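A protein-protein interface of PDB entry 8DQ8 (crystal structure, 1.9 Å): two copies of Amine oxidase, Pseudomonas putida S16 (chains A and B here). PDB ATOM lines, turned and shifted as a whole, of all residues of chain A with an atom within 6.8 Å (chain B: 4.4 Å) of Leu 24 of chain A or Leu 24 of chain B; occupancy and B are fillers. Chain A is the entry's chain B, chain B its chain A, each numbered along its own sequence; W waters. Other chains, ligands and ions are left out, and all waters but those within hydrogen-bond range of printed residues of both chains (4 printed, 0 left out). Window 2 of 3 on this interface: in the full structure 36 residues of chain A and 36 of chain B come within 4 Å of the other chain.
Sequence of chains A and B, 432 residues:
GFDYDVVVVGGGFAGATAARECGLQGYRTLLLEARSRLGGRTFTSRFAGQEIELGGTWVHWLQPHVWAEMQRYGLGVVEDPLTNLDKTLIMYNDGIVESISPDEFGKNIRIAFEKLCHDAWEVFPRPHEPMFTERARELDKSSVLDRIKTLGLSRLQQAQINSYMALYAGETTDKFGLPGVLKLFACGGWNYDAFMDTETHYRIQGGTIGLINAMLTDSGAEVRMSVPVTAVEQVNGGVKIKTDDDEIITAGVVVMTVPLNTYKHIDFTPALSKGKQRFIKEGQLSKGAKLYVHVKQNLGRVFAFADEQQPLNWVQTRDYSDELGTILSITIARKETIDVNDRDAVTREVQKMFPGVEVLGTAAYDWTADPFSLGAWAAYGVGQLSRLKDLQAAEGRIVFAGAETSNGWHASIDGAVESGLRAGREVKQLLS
The guanidinium group of Arg 72 of chain A lies within salt-bridge range of the side-chain carboxylate of Glu 21 of chain B. The side-chain amide nitrogen (NE2) of Gln 25 of chain A is in hydrogen-bond range of the side-chain carboxylate (OD1) of Asp 218 of chain B, 2.8 Å away. The side-chain amide nitrogen (NE2) of Gln 25 of chain B lies within hydrogen-bond range of the side-chain carboxylate (OD1) of Asp 218 of chain A (2.9 Å).
The side-chain carboxylate (OE2) of Glu 21 of chain B is in salt-bridge range of the guanidinium group (NH2) of Arg 20 of chain B. OH of Tyr 73 of chain A sits at hydrogen-bond distance from OD2 of Asp 218 of chain A (2.6 Å).
CD2 of Leu 24 of chain B touches O of Leu 24 of chain A, at 3.9 Å. Arg 72 of chain A touches Arg 20 of chain B (NH2 to NH2, 3.6 Å).
Glu 21 of chain A touches none of the printed residues of chain B. Leu 24 of chain A touches just one residue of chain B: Leu 24. Printed residues of chain B within 4 Å of Gln 25 of chain A: Asp 218 (2.8 Å). Gly 26 of chain A touches none of the printed residues of chain B. Printed residues of chain B within 4 Å of Arg 72 of chain A: Arg 20 (3.6 Å) and Glu 21 (3.0 Å). Printed residues of chain A within 4 Å of Arg 20 of chain B: Arg 72. Of the printed residues of chain A, Glu 21 of chain B touches Arg 72 (3.0 Å). Leu 24 of chain B touches just one residue of chain A: Leu 24. Of the printed residues of chain A, Asp 218 of chain B touches Gln 25 (2.8 Å). The nearest printed residue of chain B that does not touch Leu 24 of chain A is Gln 25 of chain B (4.6 Å). The nearest residue of chain A that does not touch Leu 24 of chain B is Gln 25 of chain A (4.6 Å). The nearest printed residue of chain B that does not touch Asp 218 of chain A is Leu 24 of chain B (6.2 Å).
Of the 15 printed residues of chain A, 4 touch a printed residue of chain B. Printed residues of chain A that touch a printed residue of chain B: Leu 24, Gln 25, Arg 72 and Asp 218. Hydrophobic or aromatic side chains of chain A within 4 Å of the printed part of chain B: Leu 24. Along chain A the printed residues that touch a printed residue of chain B span positions 24 to 218. Of the 8 printed residues of chain B, 5 touch a printed residue of chain A. Hydrophobic or aromatic side chains of chain B within 4 Å of the printed part of chain A: Leu 24. Among the printed residues, 5 pairs touch across the chains.
Leu 24 of chain B touches its own counterpart, Leu 24 of chain A. Gln 25 of chain A touches Asp 218 of chain B, and with the chains exchanged Asp 218 of chain A touches Gln 25 of chain B. Of the 5 pairs that touch across the chains among the printed residues, 3 have their exchanged pair printed and touching as well.
Water W1 bridges the backbone carbonyl oxygen (O) of Leu 24 of chain B and the backbone carbonyl oxygen (O) of Leu 24 of chain A. Water W3 lies within hydrogen-bond range of O of Asp 218 of chain B (2.9 Å) and OE1 of Gln 25 of chain A (3.2 Å). Water W4 lies within hydrogen-bond range of the side-chain carboxylate of Glu 21 of chain B (2.9 Å) and the guanidinium group of Arg 72 of chain A (3.4 Å). Water W2 bridges the backbone carbonyl oxygen of Asp 218 of chain A (2.9 Å) and the side-chain amide oxygen of Gln 25 of chain B (3.2 Å).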
ATOM      1  N   ALA A  19      17.221  18.810  -9.618  1.00  0.00           N
ATOM      2  CA  ALA A  19      16.801  19.873 -10.518  1.00  0.00           C
ATOM      3  C   ALA A  19      15.502  20.516 -10.052  1.00  0.00           C
ATOM      4  O   ALA A  19      15.332  21.724 -10.165  1.00  0.00           O
ATOM      5  CB  ALA A  19      16.627  19.283 -11.938  1.00  0.00           C
ATOM      6  N   ARG A  20      14.554  19.713  -9.571  1.00  0.00           N
ATOM      7  CA  ARG A  20      13.327  20.276  -9.006  1.00  0.00           C
ATOM      8  C   ARG A  20      13.637  21.177  -7.799  1.00  0.00           C
ATOM      9  O   ARG A  20      13.148  22.323  -7.718  1.00  0.00           O
ATOM     10  CB  ARG A  20      12.397  19.127  -8.605  1.00  0.00           C
ATOM     11  CG  ARG A  20      10.886  19.463  -8.477  1.00  0.00           C
ATOM     12  CD  ARG A  20      10.429  19.832  -7.094  1.00  0.00           C
ATOM     13  NE  ARG A  20      11.084  19.113  -5.989  1.00  0.00           N
ATOM     14  CZ  ARG A  20      10.668  17.957  -5.515  1.00  0.00           C
ATOM     15  NH1 ARG A  20       9.579  17.369  -6.009  1.00  0.00           N
ATOM     16  NH2 ARG A  20      11.380  17.353  -4.563  1.00  0.00           N
ATOM     17  N   GLU A  21      14.482  20.695  -6.874  1.00  0.00           N
ATOM     18  CA  GLU A  21      14.813  21.533  -5.700  1.00  0.00           C
ATOM     19  C   GLU A  21      15.447  22.844  -6.142  1.00  0.00           C
ATOM     20  O   GLU A  21      15.116  23.921  -5.637  1.00  0.00           O
ATOM     21  CB  GLU A  21      15.754  20.794  -4.748  1.00  0.00           C
ATOM     22  CG  GLU A  21      15.129  19.458  -4.146  1.00  0.00           C
ATOM     23  CD  GLU A  21      13.964  19.762  -3.230  1.00  0.00           C
ATOM     24  OE1 GLU A  21      14.198  20.186  -2.081  1.00  0.00           O
ATOM     25  OE2 GLU A  21      12.828  19.603  -3.647  1.00  0.00           O
ATOM     26  N   CYS A  22      16.345  22.789  -7.122  1.00  0.00           N
ATOM     27  CA  CYS A  22      17.051  24.013  -7.523  1.00  0.00           C
ATOM     28  C   CYS A  22      16.133  24.948  -8.293  1.00  0.00           C
ATOM     29  O   CYS A  22      16.172  26.176  -8.095  1.00  0.00           O
ATOM     30  CB  CYS A  22      18.278  23.654  -8.377  1.00  0.00           C
ATOM     31  SG  CYS A  22      19.583  22.830  -7.436  1.00  0.00           S
ATOM     32  N   GLY A  23      15.310  24.392  -9.191  1.00  0.00           N
ATOM     33  CA  GLY A  23      14.449  25.245 -10.007  1.00  0.00           C
ATOM     34  C   GLY A  23      13.416  25.970  -9.173  1.00  0.00           C
ATOM     35  O   GLY A  23      13.082  27.134  -9.449  1.00  0.00           O
ATOM     36  N   LEU A  24      12.877  25.291  -8.149  1.00  0.00           N
ATOM     37  CA  LEU A  24      11.885  25.972  -7.298  1.00  0.00           C
ATOM     38  C   LEU A  24      12.476  27.139  -6.501  1.00  0.00           C
ATOM     39  O   LEU A  24      11.725  28.021  -6.089  1.00  0.00           O
ATOM     40  CB  LEU A  24      11.241  24.980  -6.336  1.00  0.00           C
ATOM     41  CG  LEU A  24      10.303  23.963  -7.022  1.00  0.00           C
ATOM     42  CD1 LEU A  24       9.538  23.114  -5.969  1.00  0.00           C
ATOM     43  CD2 LEU A  24       9.349  24.595  -7.973  1.00  0.00           C
ATOM     44  N   GLN A  25      13.779  27.161  -6.259  1.00  0.00           N
ATOM     45  CA  GLN A  25      14.433  28.325  -5.649  1.00  0.00           C
ATOM     46  C   GLN A  25      14.670  29.445  -6.646  1.00  0.00           C
ATOM     47  O   GLN A  25      15.078  30.544  -6.240  1.00  0.00           O
ATOM     48  CB  GLN A  25      15.790  27.937  -5.053  1.00  0.00           C
ATOM     49  CG  GLN A  25      15.729  27.046  -3.870  1.00  0.00           C
ATOM     50  CD  GLN A  25      14.866  27.642  -2.762  1.00  0.00           C
ATOM     51  OE1 GLN A  25      15.070  28.789  -2.365  1.00  0.00           O
ATOM     52  NE2 GLN A  25      13.898  26.861  -2.269  1.00  0.00           N
ATOM     53  N   GLY A  26      14.431  29.214  -7.931  1.00  0.00           N
ATOM     54  CA  GLY A  26      14.652  30.234  -8.931  1.00  0.00           C
ATOM     55  C   GLY A  26      16.026  30.211  -9.550  1.00  0.00           C
ATOM     56  O   GLY A  26      16.356  31.119 -10.335  1.00  0.00           O
ATOM     57  N   TYR A  27      16.842  29.215  -9.236  1.00  0.00           N
ATOM     58  CA  TYR A  27      18.168  29.143  -9.841  1.00  0.00           C
ATOM     59  C   TYR A  27      18.018  28.757 -11.312  1.00  0.00           C
ATOM     60  O   TYR A  27      17.185  27.915 -11.659  1.00  0.00           O
ATOM     61  CB  TYR A  27      19.047  28.107  -9.142  1.00  0.00           C
ATOM     62  CG  TYR A  27      19.193  28.324  -7.654  1.00  0.00           C
ATOM     63  CD1 TYR A  27      19.322  29.597  -7.133  1.00  0.00           C
ATOM     64  CD2 TYR A  27      19.235  27.248  -6.794  1.00  0.00           C
ATOM     65  CE1 TYR A  27      19.473  29.791  -5.707  1.00  0.00           C
ATOM     66  CE2 TYR A  27      19.388  27.421  -5.409  1.00  0.00           C
ATOM     67  CZ  TYR A  27      19.498  28.671  -4.889  1.00  0.00           C
ATOM     68  OH  TYR A  27      19.665  28.762  -3.519  1.00  0.00           O
ATOM     69  N   THR A  29      18.728  26.627 -14.068  1.00  0.00           N
ATOM     70  CA  THR A  29      19.106  25.231 -13.930  1.00  0.00           C
ATOM     71  C   THR A  29      19.090  24.509 -15.271  1.00  0.00           C
ATOM     72  O   THR A  29      18.140  24.668 -16.057  1.00  0.00           O
ATOM     73  CB  THR A  29      18.121  24.538 -12.963  1.00  0.00           C
ATOM     74  OG1 THR A  29      18.155  25.284 -11.738  1.00  0.00           O
ATOM     75  CG2 THR A  29      18.554  23.123 -12.692  1.00  0.00           C
ATOM     76  N   ARG A  72       2.967  14.524  -2.604  1.00  0.00           N
ATOM     77  CA  ARG A  72       2.942  15.821  -3.284  1.00  0.00           C
ATOM     78  C   ARG A  72       2.276  15.736  -4.659  1.00  0.00           C
ATOM     79  O   ARG A  72       1.467  16.605  -5.020  1.00  0.00           O
ATOM     80  CB  ARG A  72       4.393  16.336  -3.426  1.00  0.00           C
ATOM     81  CG  ARG A  72       4.593  17.491  -4.410  1.00  0.00           C
ATOM     82  CD  ARG A  72       6.078  17.975  -4.427  1.00  0.00           C
ATOM     83  NE  ARG A  72       6.349  18.659  -3.137  1.00  0.00           N
ATOM     84  CZ  ARG A  72       7.147  18.178  -2.184  1.00  0.00           C
ATOM     85  NH1 ARG A  72       7.883  17.058  -2.357  1.00  0.00           N
ATOM     86  NH2 ARG A  72       7.214  18.814  -0.996  1.00  0.00           N
ATOM     87  N   TYR A  73       2.599  14.710  -5.457  1.00  0.00           N
ATOM     88  CA  TYR A  73       2.080  14.668  -6.826  1.00  0.00           C
ATOM     89  C   TYR A  73       0.807  13.837  -6.947  1.00  0.00           C
ATOM     90  O   TYR A  73       0.247  13.712  -8.049  1.00  0.00           O
ATOM     91  CB  TYR A  73       3.177  14.162  -7.787  1.00  0.00           C
ATOM     92  CG  TYR A  73       4.325  15.189  -7.857  1.00  0.00           C
ATOM     93  CD1 TYR A  73       4.143  16.416  -8.451  1.00  0.00           C
ATOM     94  CD2 TYR A  73       5.579  14.881  -7.340  1.00  0.00           C
ATOM     95  CE1 TYR A  73       5.185  17.374  -8.506  1.00  0.00           C
ATOM     96  CE2 TYR A  73       6.639  15.839  -7.349  1.00  0.00           C
ATOM     97  CZ  TYR A  73       6.431  17.069  -7.949  1.00  0.00           C
ATOM     98  OH  TYR A  73       7.445  18.005  -8.005  1.00  0.00           O
ATOM     99  N   ASP A 218       7.711  20.429 -12.932  1.00  0.00           N
ATOM    100  CA  ASP A 218       7.752  21.338 -11.785  1.00  0.00           C
ATOM    101  C   ASP A 218       9.010  22.217 -11.758  1.00  0.00           C
ATOM    102  O   ASP A 218       8.950  23.417 -11.429  1.00  0.00           O
ATOM    103  CB  ASP A 218       7.672  20.482 -10.518  1.00  0.00           C
ATOM    104  CG  ASP A 218       6.880  21.122  -9.414  1.00  0.00           C
ATOM    105  OD1 ASP A 218       6.261  22.187  -9.622  1.00  0.00           O
ATOM    106  OD2 ASP A 218       6.860  20.489  -8.330  1.00  0.00           O
ATOM    107  N   SER A 219      10.161  21.647 -12.087  1.00  0.00           N
ATOM    108  CA  SER A 219      11.440  22.310 -11.905  1.00  0.00           C
ATOM    109  C   SER A 219      11.583  23.533 -12.782  1.00  0.00           C
ATOM    110  O   SER A 219      12.225  24.514 -12.374  1.00  0.00           O
ATOM    111  CB  SER A 219      12.605  21.336 -12.182  1.00  0.00           C
ATOM    112  OG  SER A 219      12.857  21.243 -13.625  1.00  0.00           O
ATOM    113  N   GLY A 220      10.984  23.519 -13.974  1.00  0.00           N
ATOM    114  CA  GLY A 220      11.225  24.582 -14.903  1.00  0.00           C
ATOM    115  C   GLY A 220      12.601  24.561 -15.549  1.00  0.00           C
ATOM    116  O   GLY A 220      12.894  25.452 -16.367  1.00  0.00           O
ATOM    117  N   ARG B  20       3.991  26.810   1.936  1.00  0.00           N
ATOM    118  CA  ARG B  20       5.242  26.556   1.216  1.00  0.00           C
ATOM    119  C   ARG B  20       4.960  25.940  -0.171  1.00  0.00           C
ATOM    120  O   ARG B  20       5.493  26.402  -1.208  1.00  0.00           O
ATOM    121  CB  ARG B  20       6.112  25.605   2.055  1.00  0.00           C
ATOM    122  CG  ARG B  20       7.622  25.565   1.688  1.00  0.00           C
ATOM    123  CD  ARG B  20       8.020  24.497   0.683  1.00  0.00           C
ATOM    124  NE  ARG B  20       7.322  23.210   0.826  1.00  0.00           N
ATOM    125  CZ  ARG B  20       7.727  22.229   1.613  1.00  0.00           C
ATOM    126  NH1 ARG B  20       8.840  22.344   2.330  1.00  0.00           N
ATOM    127  NH2 ARG B  20       6.985  21.118   1.704  1.00  0.00           N
ATOM    128  N   GLU B  21       4.091  24.927  -0.210  1.00  0.00           N
ATOM    129  CA  GLU B  21       3.759  24.313  -1.502  1.00  0.00           C
ATOM    130  C   GLU B  21       3.184  25.354  -2.452  1.00  0.00           C
ATOM    131  O   GLU B  21       3.523  25.381  -3.641  1.00  0.00           O
ATOM    132  CB  GLU B  21       2.769  23.168  -1.334  1.00  0.00           C
ATOM    133  CG  GLU B  21       3.299  21.974  -0.470  1.00  0.00           C
ATOM    134  CD  GLU B  21       4.470  21.287  -1.151  1.00  0.00           C
ATOM    135  OE1 GLU B  21       4.243  20.507  -2.084  1.00  0.00           O
ATOM    136  OE2 GLU B  21       5.605  21.539  -0.760  1.00  0.00           O
ATOM    137  N   CYS B  22       2.302  26.225  -1.951  1.00  0.00           N
ATOM    138  CA  CYS B  22       1.657  27.181  -2.854  1.00  0.00           C
ATOM    139  C   CYS B  22       2.632  28.274  -3.281  1.00  0.00           C
ATOM    140  O   CYS B  22       2.655  28.678  -4.466  1.00  0.00           O
ATOM    141  CB  CYS B  22       0.416  27.801  -2.202  1.00  0.00           C
ATOM    142  SG  CYS B  22      -0.931  26.646  -1.919  1.00  0.00           S
ATOM    143  N   GLY B  23       3.438  28.774  -2.338  1.00  0.00           N
ATOM    144  CA  GLY B  23       4.351  29.858  -2.675  1.00  0.00           C
ATOM    145  C   GLY B  23       5.380  29.427  -3.695  1.00  0.00           C
ATOM    146  O   GLY B  23       5.762  30.209  -4.583  1.00  0.00           O
ATOM    147  N   LEU B  24       5.850  28.172  -3.594  1.00  0.00           N
ATOM    148  CA  LEU B  24       6.867  27.724  -4.570  1.00  0.00           C
ATOM    149  C   LEU B  24       6.314  27.601  -5.988  1.00  0.00           C
ATOM    150  O   LEU B  24       7.089  27.688  -6.936  1.00  0.00           O
ATOM    151  CB  LEU B  24       7.493  26.414  -4.136  1.00  0.00           C
ATOM    152  CG  LEU B  24       8.384  26.536  -2.884  1.00  0.00           C
ATOM    153  CD1 LEU B  24       9.104  25.192  -2.639  1.00  0.00           C
ATOM    154  CD2 LEU B  24       9.387  27.675  -2.957  1.00  0.00           C
ATOM    155  N   GLN B  25       5.006  27.443  -6.155  1.00  0.00           N
ATOM    156  CA  GLN B  25       4.389  27.502  -7.482  1.00  0.00           C
ATOM    157  C   GLN B  25       4.224  28.918  -7.988  1.00  0.00           C
ATOM    158  O   GLN B  25       3.901  29.109  -9.171  1.00  0.00           O
ATOM    159  CB  GLN B  25       3.005  26.836  -7.458  1.00  0.00           C
ATOM    160  CG  GLN B  25       3.032  25.375  -7.206  1.00  0.00           C
ATOM    161  CD  GLN B  25       3.896  24.641  -8.212  1.00  0.00           C
ATOM    162  OE1 GLN B  25       3.750  24.838  -9.423  1.00  0.00           O
ATOM    163  NE2 GLN B  25       4.796  23.790  -7.721  1.00  0.00           N
ATOM    164  N   GLY B  26       4.470  29.921  -7.156  1.00  0.00           N
ATOM    165  CA  GLY B  26       4.303  31.290  -7.589  1.00  0.00           C
ATOM    166  C   GLY B  26       2.949  31.879  -7.293  1.00  0.00           C
ATOM    167  O   GLY B  26       2.657  32.992  -7.746  1.00  0.00           O
ATOM    168  N   ASP B 218      11.008  29.804   3.088  1.00  0.00           N
ATOM    169  CA  ASP B 218      10.970  29.247   1.735  1.00  0.00           C
ATOM    170  C   ASP B 218       9.744  29.703   0.949  1.00  0.00           C
ATOM    171  O   ASP B 218       9.837  30.008  -0.259  1.00  0.00           O
ATOM    172  CB  ASP B 218      10.979  27.721   1.842  1.00  0.00           C
ATOM    173  CG  ASP B 218      11.784  27.059   0.776  1.00  0.00           C
ATOM    174  OD1 ASP B 218      12.497  27.734  -0.008  1.00  0.00           O
ATOM    175  OD2 ASP B 218      11.706  25.812   0.750  1.00  0.00           O
HETATM  176  O   HOH W   1       9.417  28.878  -7.182  1.00  0.00           O
HETATM  177  O   HOH W   2       6.430  24.828 -11.096  1.00  0.00           O
HETATM  178  O   HOH W   3      12.367  30.302  -1.638  1.00  0.00           O
HETATM  179  O   HOH W   4       7.950  21.828  -2.438  1.00  0.00           O
